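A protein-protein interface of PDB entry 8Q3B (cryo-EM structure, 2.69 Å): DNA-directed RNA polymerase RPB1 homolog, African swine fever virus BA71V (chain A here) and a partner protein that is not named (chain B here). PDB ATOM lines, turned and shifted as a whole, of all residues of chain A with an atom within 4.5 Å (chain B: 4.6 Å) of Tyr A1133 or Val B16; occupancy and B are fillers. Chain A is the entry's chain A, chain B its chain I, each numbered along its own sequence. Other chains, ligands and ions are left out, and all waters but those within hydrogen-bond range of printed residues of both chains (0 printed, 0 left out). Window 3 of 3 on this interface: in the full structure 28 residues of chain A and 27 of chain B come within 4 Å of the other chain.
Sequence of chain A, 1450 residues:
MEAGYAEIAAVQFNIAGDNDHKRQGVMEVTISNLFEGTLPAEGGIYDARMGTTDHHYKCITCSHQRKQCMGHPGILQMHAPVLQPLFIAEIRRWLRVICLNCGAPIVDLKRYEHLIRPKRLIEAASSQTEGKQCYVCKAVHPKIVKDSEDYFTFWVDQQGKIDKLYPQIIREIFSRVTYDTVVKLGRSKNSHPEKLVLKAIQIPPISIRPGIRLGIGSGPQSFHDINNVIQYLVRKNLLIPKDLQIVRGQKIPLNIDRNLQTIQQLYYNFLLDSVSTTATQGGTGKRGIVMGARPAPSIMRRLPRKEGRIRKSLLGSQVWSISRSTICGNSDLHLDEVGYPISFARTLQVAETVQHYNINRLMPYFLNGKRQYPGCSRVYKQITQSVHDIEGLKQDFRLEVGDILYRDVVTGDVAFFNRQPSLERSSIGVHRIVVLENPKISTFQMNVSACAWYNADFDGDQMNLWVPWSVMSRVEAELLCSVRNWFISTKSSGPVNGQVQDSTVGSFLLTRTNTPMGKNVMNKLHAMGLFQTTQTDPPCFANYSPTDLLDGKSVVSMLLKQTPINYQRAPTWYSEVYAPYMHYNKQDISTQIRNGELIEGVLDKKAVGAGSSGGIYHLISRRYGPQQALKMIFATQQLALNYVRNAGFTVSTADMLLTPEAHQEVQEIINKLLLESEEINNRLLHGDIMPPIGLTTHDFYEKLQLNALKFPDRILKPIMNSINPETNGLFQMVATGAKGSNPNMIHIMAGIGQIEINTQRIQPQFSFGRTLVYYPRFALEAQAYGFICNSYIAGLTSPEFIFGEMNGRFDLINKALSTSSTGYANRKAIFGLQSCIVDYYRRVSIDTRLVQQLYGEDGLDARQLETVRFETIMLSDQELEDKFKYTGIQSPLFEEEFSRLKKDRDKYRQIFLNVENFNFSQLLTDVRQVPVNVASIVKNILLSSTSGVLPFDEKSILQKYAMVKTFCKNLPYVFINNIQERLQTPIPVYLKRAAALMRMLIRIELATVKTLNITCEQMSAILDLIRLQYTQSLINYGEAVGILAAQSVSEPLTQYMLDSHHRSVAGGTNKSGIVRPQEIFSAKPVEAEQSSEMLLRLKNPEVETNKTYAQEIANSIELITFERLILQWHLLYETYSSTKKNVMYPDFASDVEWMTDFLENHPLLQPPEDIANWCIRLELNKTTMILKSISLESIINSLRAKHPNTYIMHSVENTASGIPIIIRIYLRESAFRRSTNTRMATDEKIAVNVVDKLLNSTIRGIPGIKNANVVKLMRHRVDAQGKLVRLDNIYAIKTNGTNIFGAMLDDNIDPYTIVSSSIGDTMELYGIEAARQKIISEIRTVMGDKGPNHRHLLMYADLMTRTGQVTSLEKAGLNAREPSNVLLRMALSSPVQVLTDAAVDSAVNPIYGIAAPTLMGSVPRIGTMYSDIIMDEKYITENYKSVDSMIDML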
ATOM      1  N   LEU A1131     -29.684  14.085  27.592  1.00  0.00           N
ATOM      2  CA  LEU A1131     -30.275  12.814  27.185  1.00  0.00           C
ATOM      3  C   LEU A1131     -29.491  11.702  27.873  1.00  0.00           C
ATOM      4  O   LEU A1131     -28.341  11.432  27.517  1.00  0.00           O
ATOM      5  CB  LEU A1131     -30.250  12.672  25.665  1.00  0.00           C
ATOM      6  CG  LEU A1131     -31.168  11.624  25.030  1.00  0.00           C
ATOM      7  CD1 LEU A1131     -32.624  11.856  25.398  1.00  0.00           C
ATOM      8  CD2 LEU A1131     -31.003  11.641  23.521  1.00  0.00           C
ATOM      9  N   LEU A1132     -30.113  11.059  28.861  1.00  0.00           N
ATOM     10  CA  LEU A1132     -29.390  10.209  29.798  1.00  0.00           C
ATOM     11  C   LEU A1132     -29.407   8.732  29.438  1.00  0.00           C
ATOM     12  O   LEU A1132     -28.495   8.003  29.841  1.00  0.00           O
ATOM     13  CB  LEU A1132     -29.971  10.375  31.208  1.00  0.00           C
ATOM     14  CG  LEU A1132     -29.714  11.697  31.938  1.00  0.00           C
ATOM     15  CD1 LEU A1132     -30.032  11.547  33.417  1.00  0.00           C
ATOM     16  CD2 LEU A1132     -28.287  12.189  31.751  1.00  0.00           C
ATOM     17  N   TYR A1133     -30.411   8.262  28.699  1.00  0.00           N
ATOM     18  CA  TYR A1133     -30.539   6.842  28.376  1.00  0.00           C
ATOM     19  C   TYR A1133     -30.639   6.006  29.655  1.00  0.00           C
ATOM     20  O   TYR A1133     -29.782   5.176  29.962  1.00  0.00           O
ATOM     21  CB  TYR A1133     -29.368   6.374  27.506  1.00  0.00           C
ATOM     22  CG  TYR A1133     -29.497   4.950  27.016  1.00  0.00           C
ATOM     23  CD1 TYR A1133     -30.565   4.561  26.221  1.00  0.00           C
ATOM     24  CD2 TYR A1133     -28.550   3.993  27.354  1.00  0.00           C
ATOM     25  CE1 TYR A1133     -30.685   3.261  25.773  1.00  0.00           C
ATOM     26  CE2 TYR A1133     -28.662   2.692  26.911  1.00  0.00           C
ATOM     27  CZ  TYR A1133     -29.731   2.331  26.122  1.00  0.00           C
ATOM     28  OH  TYR A1133     -29.846   1.034  25.679  1.00  0.00           O
ATOM     29  N   GLU A1134     -31.714   6.248  30.403  1.00  0.00           N
ATOM     30  CA  GLU A1134     -31.944   5.577  31.672  1.00  0.00           C
ATOM     31  C   GLU A1134     -33.398   5.138  31.758  1.00  0.00           C
ATOM     32  O   GLU A1134     -34.273   5.670  31.072  1.00  0.00           O
ATOM     33  CB  GLU A1134     -31.607   6.487  32.861  1.00  0.00           C
ATOM     34  CG  GLU A1134     -30.179   6.999  32.865  1.00  0.00           C
ATOM     35  CD  GLU A1134     -29.915   7.975  33.995  1.00  0.00           C
ATOM     36  OE1 GLU A1134     -30.876   8.335  34.707  1.00  0.00           O
ATOM     37  OE2 GLU A1134     -28.749   8.383  34.171  1.00  0.00           O
ATOM     38  N   ASN A1173     -36.565   3.473  28.128  1.00  0.00           N
ATOM     39  CA  ASN A1173     -35.192   3.514  28.637  1.00  0.00           C
ATOM     40  C   ASN A1173     -34.439   4.768  28.204  1.00  0.00           C
ATOM     41  O   ASN A1173     -33.218   4.841  28.407  1.00  0.00           O
ATOM     42  CB  ASN A1173     -34.393   2.277  28.209  1.00  0.00           C
ATOM     43  CG  ASN A1173     -33.074   2.147  28.944  1.00  0.00           C
ATOM     44  OD1 ASN A1173     -33.009   2.311  30.161  1.00  0.00           O
ATOM     45  ND2 ASN A1173     -32.014   1.842  28.207  1.00  0.00           N
ATOM     46  N   TRP A1174     -35.112   5.757  27.622  1.00  0.00           N
ATOM     47  CA  TRP A1174     -34.489   7.018  27.242  1.00  0.00           C
ATOM     48  C   TRP A1174     -35.056   8.136  28.104  1.00  0.00           C
ATOM     49  O   TRP A1174     -36.278   8.263  28.238  1.00  0.00           O
ATOM     50  CB  TRP A1174     -34.716   7.319  25.759  1.00  0.00           C
ATOM     51  CG  TRP A1174     -34.119   6.292  24.851  1.00  0.00           C
ATOM     52  CD1 TRP A1174     -34.643   5.073  24.537  1.00  0.00           C
ATOM     53  CD2 TRP A1174     -32.875   6.387  24.148  1.00  0.00           C
ATOM     54  NE1 TRP A1174     -33.807   4.405  23.676  1.00  0.00           N
ATOM     55  CE2 TRP A1174     -32.714   5.191  23.423  1.00  0.00           C
ATOM     56  CE3 TRP A1174     -31.884   7.368  24.060  1.00  0.00           C
ATOM     57  CZ2 TRP A1174     -31.603   4.950  22.621  1.00  0.00           C
ATOM     58  CZ3 TRP A1174     -30.783   7.127  23.262  1.00  0.00           C
ATOM     59  CH2 TRP A1174     -30.650   5.928  22.553  1.00  0.00           C
ATOM     60  N   CYS A1175     -34.170   8.942  28.684  1.00  0.00           N
ATOM     61  CA  CYS A1175     -34.546   9.980  29.632  1.00  0.00           C
ATOM     62  C   CYS A1175     -34.001  11.329  29.185  1.00  0.00           C
ATOM     63  O   CYS A1175     -32.863  11.425  28.717  1.00  0.00           O
ATOM     64  CB  CYS A1175     -34.021   9.659  31.032  1.00  0.00           C
ATOM     65  SG  CYS A1175     -34.132  11.035  32.196  1.00  0.00           S
ATOM     66  N   THR B  14     -23.277   1.320  20.956  1.00  0.00           N
ATOM     67  CA  THR B  14     -24.375   0.622  20.294  1.00  0.00           C
ATOM     68  C   THR B  14     -25.721   0.960  20.921  1.00  0.00           C
ATOM     69  O   THR B  14     -26.727   1.088  20.214  1.00  0.00           O
ATOM     70  CB  THR B  14     -24.139  -0.886  20.336  1.00  0.00           C
ATOM     71  OG1 THR B  14     -23.528  -1.240  21.581  1.00  0.00           O
ATOM     72  CG2 THR B  14     -23.235  -1.315  19.197  1.00  0.00           C
ATOM     73  N   TYR B  15     -25.766   1.098  22.247  1.00  0.00           N
ATOM     74  CA  TYR B  15     -27.017   1.325  22.971  1.00  0.00           C
ATOM     75  C   TYR B  15     -27.987   0.162  22.747  1.00  0.00           C
ATOM     76  O   TYR B  15     -29.067   0.314  22.173  1.00  0.00           O
ATOM     77  CB  TYR B  15     -27.648   2.660  22.559  1.00  0.00           C
ATOM     78  CG  TYR B  15     -26.886   3.868  23.049  1.00  0.00           C
ATOM     79  CD1 TYR B  15     -26.526   3.989  24.383  1.00  0.00           C
ATOM     80  CD2 TYR B  15     -26.530   4.888  22.179  1.00  0.00           C
ATOM     81  CE1 TYR B  15     -25.830   5.087  24.836  1.00  0.00           C
ATOM     82  CE2 TYR B  15     -25.833   5.991  22.624  1.00  0.00           C
ATOM     83  CZ  TYR B  15     -25.484   6.084  23.953  1.00  0.00           C
ATOM     84  OH  TYR B  15     -24.794   7.183  24.403  1.00  0.00           O
ATOM     85  N   VAL B  16     -27.574  -1.013  23.217  1.00  0.00           N
ATOM     86  CA  VAL B  16     -28.324  -2.251  23.042  1.00  0.00           C
ATOM     87  C   VAL B  16     -28.595  -2.861  24.409  1.00  0.00           C
ATOM     88  O   VAL B  16     -27.699  -2.919  25.259  1.00  0.00           O
ATOM     89  CB  VAL B  16     -27.570  -3.255  22.148  1.00  0.00           C
ATOM     90  CG1 VAL B  16     -27.533  -2.763  20.711  1.00  0.00           C
ATOM     91  CG2 VAL B  16     -26.158  -3.491  22.675  1.00  0.00           C
ATOM     92  N   ASP B  17     -29.833  -3.313  24.619  1.00  0.00           N
ATOM     93  CA  ASP B  17     -30.222  -4.030  25.832  1.00  0.00           C
ATOM     94  C   ASP B  17     -30.002  -3.180  27.082  1.00  0.00           C
ATOM     95  O   ASP B  17     -29.686  -3.697  28.156  1.00  0.00           O
ATOM     96  CB  ASP B  17     -29.466  -5.359  25.943  1.00  0.00           C
ATOM     97  CG  ASP B  17     -29.908  -6.191  27.133  1.00  0.00           C
ATOM     98  OD1 ASP B  17     -30.990  -5.909  27.691  1.00  0.00           O
ATOM     99  OD2 ASP B  17     -29.173  -7.129  27.510  1.00  0.00           O
ATOM    100  N   GLY B  18     -30.162  -1.864  26.955  1.00  0.00           N
ATOM    101  CA  GLY B  18     -30.013  -0.964  28.079  1.00  0.00           C
ATOM    102  C   GLY B  18     -28.597  -0.759  28.565  1.00  0.00           C
ATOM    103  O   GLY B  18     -28.364   0.163  29.358  1.00  0.00           O
ATOM    104  N   ASN B  19     -27.644  -1.577  28.129  1.00  0.00           N
ATOM    105  CA  ASN B  19     -26.249  -1.456  28.523  1.00  0.00           C
ATOM    106  C   ASN B  19     -25.427  -0.951  27.347  1.00  0.00           C
ATOM    107  O   ASN B  19     -25.605  -1.406  26.213  1.00  0.00           O
ATOM    108  CB  ASN B  19     -25.695  -2.799  29.007  1.00  0.00           C
ATOM    109  CG  ASN B  19     -25.716  -2.928  30.516  1.00  0.00           C
ATOM    110  OD1 ASN B  19     -25.275  -2.031  31.233  1.00  0.00           O
ATOM    111  ND2 ASN B  19     -26.229  -4.052  31.006  1.00  0.00           N
ATOM    112  N   ILE B  20     -24.529  -0.007  27.620  1.00  0.00           N
ATOM    113  CA  ILE B  20     -23.685   0.543  26.569  1.00  0.00           C
ATOM    114  C   ILE B  20     -22.589  -0.457  26.230  1.00  0.00           C
ATOM    115  O   ILE B  20     -21.827  -0.890  27.105  1.00  0.00           O
ATOM    116  CB  ILE B  20     -23.095   1.894  27.003  1.00  0.00           C
ATOM    117  CG1 ILE B  20     -24.143   2.999  26.873  1.00  0.00           C
ATOM    118  CG2 ILE B  20     -21.870   2.238  26.166  1.00  0.00           C
ATOM    119  CD1 ILE B  20     -25.110   3.060  28.030  1.00  0.00           C
ATOM    120  N   ILE B  21     -22.507  -0.829  24.956  1.00  0.00           N
ATOM    121  CA  ILE B  21     -21.457  -1.701  24.444  1.00  0.00           C
ATOM    122  C   ILE B  21     -20.683  -0.927  23.387  1.00  0.00           C
ATOM    123  O   ILE B  21     -21.279  -0.364  22.461  1.00  0.00           O
ATOM    124  CB  ILE B  21     -22.027  -3.010  23.868  1.00  0.00           C
ATOM    125  CG1 ILE B  21     -22.597  -3.878  24.992  1.00  0.00           C
ATOM    126  CG2 ILE B  21     -20.957  -3.769  23.088  1.00  0.00           C
ATOM    127  CD1 ILE B  21     -23.386  -5.079  24.505  1.00  0.00           C
ATOM    128  N   LEU B  37     -23.506   6.591  30.544  1.00  0.00           N
ATOM    129  CA  LEU B  37     -24.934   6.585  30.238  1.00  0.00           C
ATOM    130  C   LEU B  37     -25.337   7.809  29.424  1.00  0.00           C
ATOM    131  O   LEU B  37     -26.200   7.716  28.543  1.00  0.00           O
ATOM    132  CB  LEU B  37     -25.744   6.515  31.533  1.00  0.00           C
ATOM    133  CG  LEU B  37     -25.718   5.188  32.298  1.00  0.00           C
ATOM    134  CD1 LEU B  37     -26.659   5.246  33.487  1.00  0.00           C
ATOM    135  CD2 LEU B  37     -26.084   4.020  31.398  1.00  0.00           C
ATOM    136  N   VAL B  39     -26.108  10.259  26.825  1.00  0.00           N
ATOM    137  CA  VAL B  39     -26.080  10.206  25.366  1.00  0.00           C
ATOM    138  C   VAL B  39     -25.525  11.507  24.800  1.00  0.00           C
ATOM    139  O   VAL B  39     -24.570  11.509  24.016  1.00  0.00           O
ATOM    140  CB  VAL B  39     -27.489   9.920  24.816  1.00  0.00           C
ATOM    141  CG1 VAL B  39     -27.600  10.386  23.369  1.00  0.00           C
ATOM    142  CG2 VAL B  39     -27.834   8.449  24.950  1.00  0.00           C
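Among the printed residues, pairs that only touch across the chains: Asn A1173 with Gly B18 (3.4 Å), Tyr A1133 with Tyr B15 (3.6 Å), Tyr A1133 with Leu B37 (3.6 Å), Tyr A1133 with Ile B20 (3.6 Å), Tyr A1133 with Val B39 (3.6 Å), Trp A1174 with Val B39 (3.6 Å), Glu A1134 with Leu B37 (3.8 Å) and Tyr A1133 with Val B16 (3.9 Å).
The side-chain amide nitrogen of Asn A1173 sits close to the side-chain hydroxyl of Tyr A1133, 3.4 Å away.
O of Cys A1175 lies within hydrogen-bond range of N of Leu A1132 (2.8 Å).
The backbone carbonyl oxygen (O) of Asn A1173 sits at hydrogen-bond distance from the backbone NH (N) of Glu A1134, 2.9 Å away.
Of chain B, only Tyr B15, Val B16, Gly B18, Ile B20, Leu B37 and Val B39 come within 4 Å of Tyr A1133.
Printed residues of chain B within 4 Å of Trp A1174: Val B39 (3.6 Å).
Printed residues of chain A within 4 Å of Tyr B15: Tyr A1133.
Of the printed residues of chain A, Val B16 touches Tyr A1133.
Of the printed residues of chain A, Gly B18 touches Tyr A1133 (3.1 Å) and Asn A1173 (3.4 Å).
Of the printed residues of chain A, Leu B37 touches Leu A1132, Tyr A1133 and Glu A1134.
Printed residues of chain A within 4 Å of Val B39: Leu A1131 (2.6 Å), Tyr A1133 (3.6 Å) and Trp A1174 (3.6 Å).
The nearest printed residue of chain A that does not touch Gly B18 is Glu A1134 (6.9 Å).
Of the 7 printed residues of chain A, 6 touch a printed residue of chain B.
Printed residues of chain A that touch a printed residue of chain B: Leu A1131, Leu A1132, Tyr A1133, Glu A1134, Asn A1173 and Trp A1174.
Of the 10 printed residues of chain B, 6 touch a printed residue of chain A.
Among the printed residues, no Asp or Glu carboxylate lies within 4 Å of a Lys or Arg side-chain nitrogen of the other chain.
The backbone carbonyl oxygen of Leu A1132 lies close to the backbone carbonyl oxygen of Leu B37, at 2.7 Å.
The side-chain hydroxyl (OH) of Tyr A1133 sits close to the backbone NH (N) of Gly B18 (3.2 Å).
The backbone carbonyl oxygen (O) of Leu A1131 is in hydrogen-bond range of the backbone NH (N) of Val B39.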
